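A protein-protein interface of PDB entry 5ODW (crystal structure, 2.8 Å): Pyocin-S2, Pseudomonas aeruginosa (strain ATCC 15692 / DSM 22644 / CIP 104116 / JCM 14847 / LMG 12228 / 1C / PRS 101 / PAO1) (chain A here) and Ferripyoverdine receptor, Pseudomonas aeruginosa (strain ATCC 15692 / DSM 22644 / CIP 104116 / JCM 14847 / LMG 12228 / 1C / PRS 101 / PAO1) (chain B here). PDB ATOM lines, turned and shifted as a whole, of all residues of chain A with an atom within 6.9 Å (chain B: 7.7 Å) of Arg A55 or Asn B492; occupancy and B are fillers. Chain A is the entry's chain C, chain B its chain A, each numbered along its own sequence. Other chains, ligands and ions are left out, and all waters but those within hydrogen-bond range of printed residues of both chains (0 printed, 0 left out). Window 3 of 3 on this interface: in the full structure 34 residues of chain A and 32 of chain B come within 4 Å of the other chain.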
ATOM      1  N   VAL A  47     -10.078   8.946   6.828  1.00  0.00           N
ATOM      2  CA  VAL A  47     -11.297   9.694   7.181  1.00  0.00           C
ATOM      3  C   VAL A  47     -12.535   8.751   7.270  1.00  0.00           C
ATOM      4  O   VAL A  47     -13.133   8.644   8.346  1.00  0.00           O
ATOM      5  CB  VAL A  47     -11.546  10.958   6.311  1.00  0.00           C
ATOM      6  CG1 VAL A  47     -12.758  11.721   6.818  1.00  0.00           C
ATOM      7  CG2 VAL A  47     -10.333  11.874   6.323  1.00  0.00           C
ATOM      8  N   GLY A  48     -12.838   8.046   6.175  1.00  0.00           N
ATOM      9  CA  GLY A  48     -13.947   7.101   6.079  1.00  0.00           C
ATOM     10  C   GLY A  48     -14.024   6.123   7.228  1.00  0.00           C
ATOM     11  O   GLY A  48     -15.057   6.052   7.903  1.00  0.00           O
ATOM     12  N   THR A  49     -12.913   5.386   7.474  1.00  0.00           N
ATOM     13  CA  THR A  49     -12.816   4.388   8.553  1.00  0.00           C
ATOM     14  C   THR A  49     -12.761   5.066   9.937  1.00  0.00           C
ATOM     15  O   THR A  49     -13.276   4.506  10.903  1.00  0.00           O
ATOM     16  CB  THR A  49     -11.677   3.375   8.310  1.00  0.00           C
ATOM     17  OG1 THR A  49     -10.429   4.055   8.299  1.00  0.00           O
ATOM     18  CG2 THR A  49     -11.844   2.588   7.008  1.00  0.00           C
ATOM     19  N   GLY A  50     -12.213   6.283   9.997  1.00  0.00           N
ATOM     20  CA  GLY A  50     -12.154   7.074  11.223  1.00  0.00           C
ATOM     21  C   GLY A  50     -13.525   7.480  11.719  1.00  0.00           C
ATOM     22  O   GLY A  50     -13.818   7.397  12.918  1.00  0.00           O
ATOM     23  N   MET A  51     -14.376   7.896  10.772  1.00  0.00           N
ATOM     24  CA  MET A  51     -15.754   8.303  11.013  1.00  0.00           C
ATOM     25  C   MET A  51     -16.608   7.099  11.412  1.00  0.00           C
ATOM     26  O   MET A  51     -17.421   7.205  12.340  1.00  0.00           O
ATOM     27  CB  MET A  51     -16.319   9.044   9.788  1.00  0.00           C
ATOM     28  CG  MET A  51     -15.776  10.494   9.611  1.00  0.00           C
ATOM     29  SD  MET A  51     -15.460  11.533  11.096  1.00  0.00           S
ATOM     30  CE  MET A  51     -17.128  11.844  11.668  1.00  0.00           C
ATOM     31  N   GLN A  52     -16.363   5.937  10.736  1.00  0.00           N
ATOM     32  CA  GLN A  52     -16.967   4.610  10.940  1.00  0.00           C
ATOM     33  C   GLN A  52     -16.628   4.090  12.352  1.00  0.00           C
ATOM     34  O   GLN A  52     -17.510   3.548  13.019  1.00  0.00           O
ATOM     35  CB  GLN A  52     -16.425   3.641   9.873  1.00  0.00           C
ATOM     36  CG  GLN A  52     -17.022   2.235   9.871  1.00  0.00           C
ATOM     37  CD  GLN A  52     -16.109   1.247   9.166  1.00  0.00           C
ATOM     38  OE1 GLN A  52     -15.785   1.391   7.970  1.00  0.00           O
ATOM     39  NE2 GLN A  52     -15.664   0.218   9.894  1.00  0.00           N
ATOM     40  N   GLU A  53     -15.359   4.244  12.800  1.00  0.00           N
ATOM     41  CA  GLU A  53     -14.899   3.797  14.121  1.00  0.00           C
ATOM     42  C   GLU A  53     -15.457   4.675  15.235  1.00  0.00           C
ATOM     43  O   GLU A  53     -15.722   4.173  16.334  1.00  0.00           O
ATOM     44  CB  GLU A  53     -13.362   3.724  14.197  1.00  0.00           C
ATOM     45  CG  GLU A  53     -12.723   2.592  13.401  1.00  0.00           C
ATOM     46  CD  GLU A  53     -13.286   1.212  13.673  1.00  0.00           C
ATOM     47  OE1 GLU A  53     -13.140   0.723  14.818  1.00  0.00           O
ATOM     48  OE2 GLU A  53     -13.893   0.628  12.745  1.00  0.00           O
ATOM     49  N   TYR A  54     -15.642   5.985  14.943  1.00  0.00           N
ATOM     50  CA  TYR A  54     -16.198   6.978  15.861  1.00  0.00           C
ATOM     51  C   TYR A  54     -17.645   6.654  16.150  1.00  0.00           C
ATOM     52  O   TYR A  54     -18.027   6.579  17.312  1.00  0.00           O
ATOM     53  CB  TYR A  54     -16.079   8.397  15.279  1.00  0.00           C
ATOM     54  CG  TYR A  54     -16.578   9.478  16.219  1.00  0.00           C
ATOM     55  CD1 TYR A  54     -17.929   9.812  16.273  1.00  0.00           C
ATOM     56  CD2 TYR A  54     -15.700  10.161  17.061  1.00  0.00           C
ATOM     57  CE1 TYR A  54     -18.402  10.765  17.165  1.00  0.00           C
ATOM     58  CE2 TYR A  54     -16.159  11.141  17.936  1.00  0.00           C
ATOM     59  CZ  TYR A  54     -17.511  11.434  17.988  1.00  0.00           C
ATOM     60  OH  TYR A  54     -17.980  12.396  18.839  1.00  0.00           O
ATOM     61  N   ARG A  55     -18.454   6.484  15.101  1.00  0.00           N
ATOM     62  CA  ARG A  55     -19.875   6.162  15.207  1.00  0.00           C
ATOM     63  C   ARG A  55     -20.093   4.865  16.032  1.00  0.00           C
ATOM     64  O   ARG A  55     -20.999   4.838  16.877  1.00  0.00           O
ATOM     65  CB  ARG A  55     -20.520   6.103  13.804  1.00  0.00           C
ATOM     66  CG  ARG A  55     -20.712   7.484  13.167  1.00  0.00           C
ATOM     67  CD  ARG A  55     -21.200   7.417  11.737  1.00  0.00           C
ATOM     68  NE  ARG A  55     -20.078   7.401  10.794  1.00  0.00           N
ATOM     69  CZ  ARG A  55     -20.203   7.448   9.469  1.00  0.00           C
ATOM     70  NH1 ARG A  55     -21.405   7.540   8.911  1.00  0.00           N
ATOM     71  NH2 ARG A  55     -19.127   7.400   8.693  1.00  0.00           N
ATOM     72  N   LYS A  56     -19.203   3.836  15.855  1.00  0.00           N
ATOM     73  CA  LYS A  56     -19.224   2.553  16.593  1.00  0.00           C
ATOM     74  C   LYS A  56     -19.005   2.764  18.092  1.00  0.00           C
ATOM     75  O   LYS A  56     -19.802   2.293  18.915  1.00  0.00           O
ATOM     76  CB  LYS A  56     -18.179   1.560  16.054  1.00  0.00           C
ATOM     77  CG  LYS A  56     -18.607   0.864  14.767  1.00  0.00           C
ATOM     78  CD  LYS A  56     -17.750  -0.356  14.471  1.00  0.00           C
ATOM     79  CE  LYS A  56     -17.584  -0.557  12.984  1.00  0.00           C
ATOM     80  NZ  LYS A  56     -16.523  -1.552  12.669  1.00  0.00           N
ATOM     81  N   LEU A  57     -17.928   3.486  18.447  1.00  0.00           N
ATOM     82  CA  LEU A  57     -17.584   3.732  19.852  1.00  0.00           C
ATOM     83  C   LEU A  57     -18.508   4.721  20.556  1.00  0.00           C
ATOM     84  O   LEU A  57     -18.842   4.503  21.727  1.00  0.00           O
ATOM     85  CB  LEU A  57     -16.124   4.161  19.986  1.00  0.00           C
ATOM     86  CG  LEU A  57     -15.103   3.037  19.922  1.00  0.00           C
ATOM     87  CD1 LEU A  57     -13.800   3.540  19.373  1.00  0.00           C
ATOM     88  CD2 LEU A  57     -14.902   2.391  21.277  1.00  0.00           C
ATOM     89  N   ARG A  58     -18.909   5.804  19.858  1.00  0.00           N
ATOM     90  CA  ARG A  58     -19.794   6.843  20.391  1.00  0.00           C
ATOM     91  C   ARG A  58     -21.113   6.260  20.853  1.00  0.00           C
ATOM     92  O   ARG A  58     -21.523   6.598  21.957  1.00  0.00           O
ATOM     93  CB  ARG A  58     -19.985   8.020  19.405  1.00  0.00           C
ATOM     94  CG  ARG A  58     -20.873   9.181  19.898  1.00  0.00           C
ATOM     95  CD  ARG A  58     -20.216  10.126  20.901  1.00  0.00           C
ATOM     96  NE  ARG A  58     -21.204  10.983  21.561  1.00  0.00           N
ATOM     97  CZ  ARG A  58     -21.268  12.306  21.452  1.00  0.00           C
ATOM     98  NH1 ARG A  58     -20.395  12.962  20.696  1.00  0.00           N
ATOM     99  NH2 ARG A  58     -22.203  12.986  22.103  1.00  0.00           N
ATOM    100  N   SER A  59     -21.754   5.356  20.079  1.00  0.00           N
ATOM    101  CA  SER A  59     -23.022   4.724  20.501  1.00  0.00           C
ATOM    102  C   SER A  59     -22.902   3.891  21.817  1.00  0.00           C
ATOM    103  O   SER A  59     -23.692   4.111  22.743  1.00  0.00           O
ATOM    104  CB  SER A  59     -23.627   3.896  19.373  1.00  0.00           C
ATOM    105  OG  SER A  59     -22.623   3.146  18.713  1.00  0.00           O
ATOM    106  N   THR A  60     -21.860   3.020  21.921  1.00  0.00           N
ATOM    107  CA  THR A  60     -21.556   2.177  23.093  1.00  0.00           C
ATOM    108  C   THR A  60     -21.224   2.954  24.360  1.00  0.00           C
ATOM    109  O   THR A  60     -21.353   2.407  25.456  1.00  0.00           O
ATOM    110  CB  THR A  60     -20.439   1.192  22.791  1.00  0.00           C
ATOM    111  OG1 THR A  60     -19.457   1.864  22.018  1.00  0.00           O
ATOM    112  CG2 THR A  60     -20.931  -0.036  22.042  1.00  0.00           C
ATOM    113  N   GLU A 138     -18.243  15.192  17.530  1.00  0.00           N
ATOM    114  CA  GLU A 138     -18.206  14.643  16.167  1.00  0.00           C
ATOM    115  C   GLU A 138     -17.718  15.627  15.102  1.00  0.00           C
ATOM    116  O   GLU A 138     -16.942  15.266  14.226  1.00  0.00           O
ATOM    117  CB  GLU A 138     -19.543  14.012  15.764  1.00  0.00           C
ATOM    118  CG  GLU A 138     -19.477  13.272  14.435  1.00  0.00           C
ATOM    119  CD  GLU A 138     -20.534  12.196  14.294  1.00  0.00           C
ATOM    120  OE1 GLU A 138     -20.660  11.623  13.194  1.00  0.00           O
ATOM    121  OE2 GLU A 138     -21.236  11.915  15.280  1.00  0.00           O
ATOM    122  N   TYR A 141     -13.811  16.246  15.723  1.00  0.00           N
ATOM    123  CA  TYR A 141     -13.075  15.040  15.338  1.00  0.00           C
ATOM    124  C   TYR A 141     -12.846  14.994  13.831  1.00  0.00           C
ATOM    125  O   TYR A 141     -11.710  14.829  13.384  1.00  0.00           O
ATOM    126  CB  TYR A 141     -13.828  13.789  15.836  1.00  0.00           C
ATOM    127  CG  TYR A 141     -13.271  12.442  15.409  1.00  0.00           C
ATOM    128  CD1 TYR A 141     -12.195  11.865  16.078  1.00  0.00           C
ATOM    129  CD2 TYR A 141     -13.903  11.686  14.423  1.00  0.00           C
ATOM    130  CE1 TYR A 141     -11.722  10.598  15.733  1.00  0.00           C
ATOM    131  CE2 TYR A 141     -13.444  10.419  14.075  1.00  0.00           C
ATOM    132  CZ  TYR A 141     -12.359   9.873  14.740  1.00  0.00           C
ATOM    133  OH  TYR A 141     -11.911   8.616  14.405  1.00  0.00           O
ATOM    134  N   GLN A 142     -13.916  15.171  13.057  1.00  0.00           N
ATOM    135  CA  GLN A 142     -13.866  15.154  11.602  1.00  0.00           C
ATOM    136  C   GLN A 142     -12.981  16.280  11.078  1.00  0.00           C
ATOM    137  O   GLN A 142     -12.247  16.052  10.126  1.00  0.00           O
ATOM    138  CB  GLN A 142     -15.277  15.224  11.006  1.00  0.00           C
ATOM    139  CG  GLN A 142     -15.322  14.891   9.520  1.00  0.00           C
ATOM    140  CD  GLN A 142     -16.614  15.277   8.868  1.00  0.00           C
ATOM    141  OE1 GLN A 142     -17.320  14.441   8.298  1.00  0.00           O
ATOM    142  NE2 GLN A 142     -16.953  16.552   8.933  1.00  0.00           N
ATOM    143  N   LEU A 156      -9.449   9.612  18.083  1.00  0.00           N
ATOM    144  CA  LEU A 156     -10.535   8.767  18.532  1.00  0.00           C
ATOM    145  C   LEU A 156     -10.370   8.401  20.008  1.00  0.00           C
ATOM    146  O   LEU A 156     -11.338   8.531  20.759  1.00  0.00           O
ATOM    147  CB  LEU A 156     -10.617   7.525  17.626  1.00  0.00           C
ATOM    148  CG  LEU A 156     -11.656   6.446  17.955  1.00  0.00           C
ATOM    149  CD1 LEU A 156     -13.088   6.973  17.850  1.00  0.00           C
ATOM    150  CD2 LEU A 156     -11.475   5.265  17.048  1.00  0.00           C
ATOM    151  N   ALA B 445     -12.445   1.932   0.450  1.00  0.00           N
ATOM    152  CA  ALA B 445     -12.950   2.526  -0.793  1.00  0.00           C
ATOM    153  C   ALA B 445     -13.491   3.946  -0.568  1.00  0.00           C
ATOM    154  O   ALA B 445     -14.335   4.153   0.305  1.00  0.00           O
ATOM    155  CB  ALA B 445     -14.019   1.630  -1.435  1.00  0.00           C
ATOM    156  N   GLN B 446     -12.972   4.924  -1.330  1.00  0.00           N
ATOM    157  CA  GLN B 446     -13.393   6.326  -1.307  1.00  0.00           C
ATOM    158  C   GLN B 446     -13.331   6.863  -2.735  1.00  0.00           C
ATOM    159  O   GLN B 446     -12.418   6.489  -3.483  1.00  0.00           O
ATOM    160  CB  GLN B 446     -12.519   7.165  -0.358  1.00  0.00           C
ATOM    161  CG  GLN B 446     -12.815   6.951   1.138  1.00  0.00           C
ATOM    162  CD  GLN B 446     -11.883   7.640   2.118  1.00  0.00           C
ATOM    163  OE1 GLN B 446     -11.183   8.602   1.805  1.00  0.00           O
ATOM    164  NE2 GLN B 446     -11.879   7.162   3.353  1.00  0.00           N
ATOM    165  N   LYS B 447     -14.272   7.743  -3.062  1.00  0.00           N
ATOM    166  CA  LYS B 447     -14.392   8.347  -4.377  1.00  0.00           C
ATOM    167  C   LYS B 447     -14.175   9.859  -4.327  1.00  0.00           C
ATOM    168  O   LYS B 447     -14.793  10.559  -3.538  1.00  0.00           O
ATOM    169  CB  LYS B 447     -15.771   8.021  -4.943  1.00  0.00           C
ATOM    170  CG  LYS B 447     -16.043   8.502  -6.353  1.00  0.00           C
ATOM    171  CD  LYS B 447     -17.325   7.872  -6.863  1.00  0.00           C
ATOM    172  CE  LYS B 447     -17.701   8.357  -8.248  1.00  0.00           C
ATOM    173  NZ  LYS B 447     -18.424   9.652  -8.199  1.00  0.00           N
ATOM    174  N   SER B 489     -16.223  14.630  -2.443  1.00  0.00           N
ATOM    175  CA  SER B 489     -15.495  13.523  -1.830  1.00  0.00           C
ATOM    176  C   SER B 489     -16.506  12.597  -1.129  1.00  0.00           C
ATOM    177  O   SER B 489     -17.333  13.100  -0.362  1.00  0.00           O
ATOM    178  CB  SER B 489     -14.454  14.067  -0.865  1.00  0.00           C
ATOM    179  OG  SER B 489     -13.739  13.007  -0.265  1.00  0.00           O
ATOM    180  N   TYR B 490     -16.496  11.269  -1.454  1.00  0.00           N
ATOM    181  CA  TYR B 490     -17.452  10.282  -0.929  1.00  0.00           C
ATOM    182  C   TYR B 490     -16.784   9.252  -0.032  1.00  0.00           C
ATOM    183  O   TYR B 490     -15.931   8.517  -0.514  1.00  0.00           O
ATOM    184  CB  TYR B 490     -18.182   9.556  -2.068  1.00  0.00           C
ATOM    185  CG  TYR B 490     -18.778  10.429  -3.155  1.00  0.00           C
ATOM    186  CD1 TYR B 490     -17.970  11.017  -4.123  1.00  0.00           C
ATOM    187  CD2 TYR B 490     -20.152  10.541  -3.307  1.00  0.00           C
ATOM    188  CE1 TYR B 490     -18.508  11.780  -5.156  1.00  0.00           C
ATOM    189  CE2 TYR B 490     -20.705  11.290  -4.347  1.00  0.00           C
ATOM    190  CZ  TYR B 490     -19.877  11.907  -5.272  1.00  0.00           C
ATOM    191  OH  TYR B 490     -20.387  12.647  -6.311  1.00  0.00           O
ATOM    192  N   TRP B 491     -17.146   9.200   1.269  1.00  0.00           N
ATOM    193  CA  TRP B 491     -16.572   8.235   2.231  1.00  0.00           C
ATOM    194  C   TRP B 491     -17.624   7.601   3.149  1.00  0.00           C
ATOM    195  O   TRP B 491     -17.250   6.868   4.071  1.00  0.00           O
ATOM    196  CB  TRP B 491     -15.409   8.827   3.050  1.00  0.00           C
ATOM    197  CG  TRP B 491     -15.773   9.938   4.013  1.00  0.00           C
ATOM    198  CD1 TRP B 491     -16.462   9.821   5.186  1.00  0.00           C
ATOM    199  CD2 TRP B 491     -15.297  11.293   3.966  1.00  0.00           C
ATOM    200  NE1 TRP B 491     -16.530  11.043   5.822  1.00  0.00           N
ATOM    201  CE2 TRP B 491     -15.810  11.959   5.105  1.00  0.00           C
ATOM    202  CE3 TRP B 491     -14.537  12.027   3.031  1.00  0.00           C
ATOM    203  CZ2 TRP B 491     -15.600  13.319   5.331  1.00  0.00           C
ATOM    204  CZ3 TRP B 491     -14.297  13.365   3.277  1.00  0.00           C
ATOM    205  CH2 TRP B 491     -14.835  14.003   4.408  1.00  0.00           C
ATOM    206  N   ASN B 492     -18.927   7.905   2.932  1.00  0.00           N
ATOM    207  CA  ASN B 492     -20.014   7.317   3.713  1.00  0.00           C
ATOM    208  C   ASN B 492     -20.764   6.373   2.778  1.00  0.00           C
ATOM    209  O   ASN B 492     -21.765   6.751   2.166  1.00  0.00           O
ATOM    210  CB  ASN B 492     -20.923   8.385   4.317  1.00  0.00           C
ATOM    211  CG  ASN B 492     -20.226   9.444   5.139  1.00  0.00           C
ATOM    212  OD1 ASN B 492     -20.235  10.625   4.773  1.00  0.00           O
ATOM    213  ND2 ASN B 492     -19.671   9.074   6.296  1.00  0.00           N
ATOM    214  N   LEU B 493     -20.212   5.166   2.612  1.00  0.00           N
ATOM    215  CA  LEU B 493     -20.711   4.126   1.708  1.00  0.00           C
ATOM    216  C   LEU B 493     -21.930   3.399   2.266  1.00  0.00           C
ATOM    217  O   LEU B 493     -22.025   3.168   3.475  1.00  0.00           O
ATOM    218  CB  LEU B 493     -19.598   3.117   1.347  1.00  0.00           C
ATOM    219  CG  LEU B 493     -18.189   3.689   1.110  1.00  0.00           C
ATOM    220  CD1 LEU B 493     -17.143   2.606   1.183  1.00  0.00           C
ATOM    221  CD2 LEU B 493     -18.101   4.428  -0.190  1.00  0.00           C
ATOM    222  N   ARG B 494     -22.856   3.027   1.376  1.00  0.00           N
ATOM    223  CA  ARG B 494     -24.082   2.351   1.750  1.00  0.00           C
ATOM    224  C   ARG B 494     -23.910   0.846   1.784  1.00  0.00           C
ATOM    225  O   ARG B 494     -23.537   0.249   0.766  1.00  0.00           O
ATOM    226  CB  ARG B 494     -25.221   2.758   0.798  1.00  0.00           C
ATOM    227  CG  ARG B 494     -26.041   3.979   1.250  1.00  0.00           C
ATOM    228  CD  ARG B 494     -27.521   3.879   0.904  1.00  0.00           C
ATOM    229  NE  ARG B 494     -28.162   2.735   1.564  1.00  0.00           N
ATOM    230  CZ  ARG B 494     -29.379   2.283   1.279  1.00  0.00           C
ATOM    231  NH1 ARG B 494     -30.117   2.877   0.348  1.00  0.00           N
ATOM    232  NH2 ARG B 494     -29.870   1.233   1.922  1.00  0.00           N
ATOM    233  N   ASN B 495     -24.149   0.225   2.939  1.00  0.00           N
ATOM    234  CA  ASN B 495     -24.226  -1.242   3.030  1.00  0.00           C
ATOM    235  C   ASN B 495     -23.129  -2.012   2.318  1.00  0.00           C
ATOM    236  O   ASN B 495     -23.424  -2.906   1.530  1.00  0.00           O
ATOM    237  CB  ASN B 495     -25.579  -1.725   2.496  1.00  0.00           C
ATOM    238  CG  ASN B 495     -26.755  -1.007   3.131  1.00  0.00           C
ATOM    239  OD1 ASN B 495     -27.632  -0.499   2.435  1.00  0.00           O
ATOM    240  ND2 ASN B 495     -26.780  -0.968   4.456  1.00  0.00           N
ATOM    241  N   PRO B 513     -18.748  -0.293  -4.213  1.00  0.00           N
ATOM    242  CA  PRO B 513     -19.782   0.164  -3.262  1.00  0.00           C
ATOM    243  C   PRO B 513     -20.788   1.211  -3.793  1.00  0.00           C
ATOM    244  O   PRO B 513     -20.547   1.855  -4.835  1.00  0.00           O
ATOM    245  CB  PRO B 513     -18.951   0.728  -2.095  1.00  0.00           C
ATOM    246  CG  PRO B 513     -17.661   1.103  -2.671  1.00  0.00           C
ATOM    247  CD  PRO B 513     -17.461   0.391  -3.975  1.00  0.00           C
ATOM    248  N   ASP B 514     -21.930   1.401  -3.055  1.00  0.00           N
ATOM    249  CA  ASP B 514     -22.871   2.494  -3.341  1.00  0.00           C
ATOM    250  C   ASP B 514     -22.244   3.639  -2.543  1.00  0.00           C
ATOM    251  O   ASP B 514     -22.300   3.643  -1.308  1.00  0.00           O
ATOM    252  CB  ASP B 514     -24.323   2.186  -2.895  1.00  0.00           C
ATOM    253  CG  ASP B 514     -25.287   3.387  -2.833  1.00  0.00           C
ATOM    254  OD1 ASP B 514     -24.974   4.439  -3.428  1.00  0.00           O
ATOM    255  OD2 ASP B 514     -26.368   3.258  -2.199  1.00  0.00           O
ATOM    256  N   TRP B 515     -21.549   4.549  -3.259  1.00  0.00           N
ATOM    257  CA  TRP B 515     -20.752   5.676  -2.717  1.00  0.00           C
ATOM    258  C   TRP B 515     -21.532   6.615  -1.820  1.00  0.00           C
ATOM    259  O   TRP B 515     -20.942   7.434  -1.093  1.00  0.00           O
ATOM    260  CB  TRP B 515     -20.063   6.479  -3.848  1.00  0.00           C
ATOM    261  CG  TRP B 515     -19.210   5.633  -4.744  1.00  0.00           C
ATOM    262  CD1 TRP B 515     -19.542   5.147  -5.972  1.00  0.00           C
ATOM    263  CD2 TRP B 515     -17.915   5.098  -4.435  1.00  0.00           C
ATOM    264  NE1 TRP B 515     -18.513   4.384  -6.473  1.00  0.00           N
ATOM    265  CE2 TRP B 515     -17.503   4.334  -5.549  1.00  0.00           C
ATOM    266  CE3 TRP B 515     -17.050   5.211  -3.331  1.00  0.00           C
ATOM    267  CZ2 TRP B 515     -16.269   3.681  -5.590  1.00  0.00           C
ATOM    268  CZ3 TRP B 515     -15.843   4.543  -3.361  1.00  0.00           C
ATOM    269  CH2 TRP B 515     -15.456   3.797  -4.485  1.00  0.00           C
ATOM    270  N   GLY B 516     -22.850   6.502  -1.899  1.00  0.00           N
ATOM    271  CA  GLY B 516     -23.762   7.361  -1.174  1.00  0.00           C
ATOM    272  C   GLY B 516     -23.739   8.762  -1.758  1.00  0.00           C
ATOM    273  O   GLY B 516     -23.654   8.944  -2.981  1.00  0.00           O
ATOM    274  N   THR B 517     -23.768   9.747  -0.864  1.00  0.00           N
ATOM    275  CA  THR B 517     -23.816  11.169  -1.158  1.00  0.00           C
ATOM    276  C   THR B 517     -22.483  11.871  -0.764  1.00  0.00           C
ATOM    277  O   THR B 517     -21.757  11.324   0.091  1.00  0.00           O
ATOM    278  CB  THR B 517     -25.078  11.753  -0.518  1.00  0.00           C
ATOM    279  OG1 THR B 517     -25.314  13.022  -1.097  1.00  0.00           O
ATOM    280  CG2 THR B 517     -25.002  11.865   0.999  1.00  0.00           C
ATOM    281  N   PRO B 518     -22.109  13.040  -1.380  1.00  0.00           N
ATOM    282  CA  PRO B 518     -20.830  13.676  -1.016  1.00  0.00           C
ATOM    283  C   PRO B 518     -20.713  13.986   0.473  1.00  0.00           C
ATOM    284  O   PRO B 518     -21.645  14.505   1.088  1.00  0.00           O
ATOM    285  CB  PRO B 518     -20.774  14.931  -1.913  1.00  0.00           C
ATOM    286  CG  PRO B 518     -21.670  14.638  -3.013  1.00  0.00           C
ATOM    287  CD  PRO B 518     -22.779  13.818  -2.439  1.00  0.00           C
ATOM    288  N   SER B 519     -19.574  13.582   1.047  1.00  0.00           N
ATOM    289  CA  SER B 519     -19.168  13.723   2.446  1.00  0.00           C
ATOM    290  C   SER B 519     -18.396  15.027   2.679  1.00  0.00           C
ATOM    291  O   SER B 519     -18.179  15.421   3.832  1.00  0.00           O
ATOM    292  CB  SER B 519     -18.285  12.549   2.836  1.00  0.00           C
ATOM    293  OG  SER B 519     -18.802  11.319   2.354  1.00  0.00           O
ATOM    294  N   GLN B 520     -17.963  15.680   1.578  1.00  0.00           N
ATOM    295  CA  GLN B 520     -17.181  16.924   1.555  1.00  0.00           C
ATOM    296  C   GLN B 520     -17.232  17.522   0.147  1.00  0.00           C
ATOM    297  O   GLN B 520     -17.258  16.784  -0.832  1.00  0.00           O
ATOM    298  CB  GLN B 520     -15.730  16.628   1.946  1.00  0.00           C
ATOM    299  CG  GLN B 520     -14.866  17.848   2.211  1.00  0.00           C
ATOM    300  CD  GLN B 520     -13.401  17.502   2.096  1.00  0.00           C
ATOM    301  OE1 GLN B 520     -13.017  16.442   1.588  1.00  0.00           O
ATOM    302  NE2 GLN B 520     -12.538  18.393   2.550  1.00  0.00           N
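The side-chain amide nitrogen (NE2) of Gln B446 lies close to the backbone NH (N) of Gly A48 (3.1 Å).
NH2 of Arg A55 sits close to ND2 of Asn B492.
O of Arg A55 lies within hydrogen-bond range of OG of Ser A59.
The backbone carbonyl oxygen of Met A51 is in hydrogen-bond range of the guanidinium group of Arg A55 (3.1 Å).
The backbone NH (N) of Trp B491 sits at hydrogen-bond distance from the side-chain hydroxyl (OG) of Ser B519, 2.9 Å away.
OD1 of Asn B492 is in hydrogen-bond range of OG of Ser B519, 2.9 Å away.
Among the printed residues, merely in contact across the chains: Val A47 with Trp B491 (3.5 Å), Gly A48 with Trp B491 (3.8 Å), Met A51 with Trp B491 (3.9 Å) and Gln A142 with Trp B491 (3.6 Å).
Of chain B, only Asn B492 comes within 4 Å of Arg A55.
Printed residues of chain A within 4 Å of Trp B491: Val A47, Gly A48, Met A51 and Gln A142.
Of the printed residues of chain B, Gln A142 touches Trp B491.
Of the printed residues of chain A, Gln B446 touches Gly A48 (3.1 Å).
Of the printed residues of chain B, Met A51 touches Trp B491.
Of the printed residues of chain B, Val A47 touches Trp B491 (3.5 Å).
The nearest residue of chain B that does not touch Arg A55 is Trp B491 (5.0 Å).
The nearest residue of chain A that does not touch Asn B492 is Met A51 (4.8 Å).
The nearest printed residue of chain B that does not touch Val A47 is Gln B446 (4.3 Å).
Of the 18 printed residues of chain A, 5 touch a printed residue of chain B.
Hydrophobic or aromatic side chains of chain A that line the printed part of chain B: Val A47 and Met A51.
Printed residues of chain B that touch a printed residue of chain A: Gln B446, Trp B491 and Asn B492.
Along chain B the printed residues that touch a printed residue of chain A span positions 446 to 492.
Among the printed residues, no Asp or Glu carboxylate lies within 4 Å of a Lys or Arg side-chain nitrogen of the other chain.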
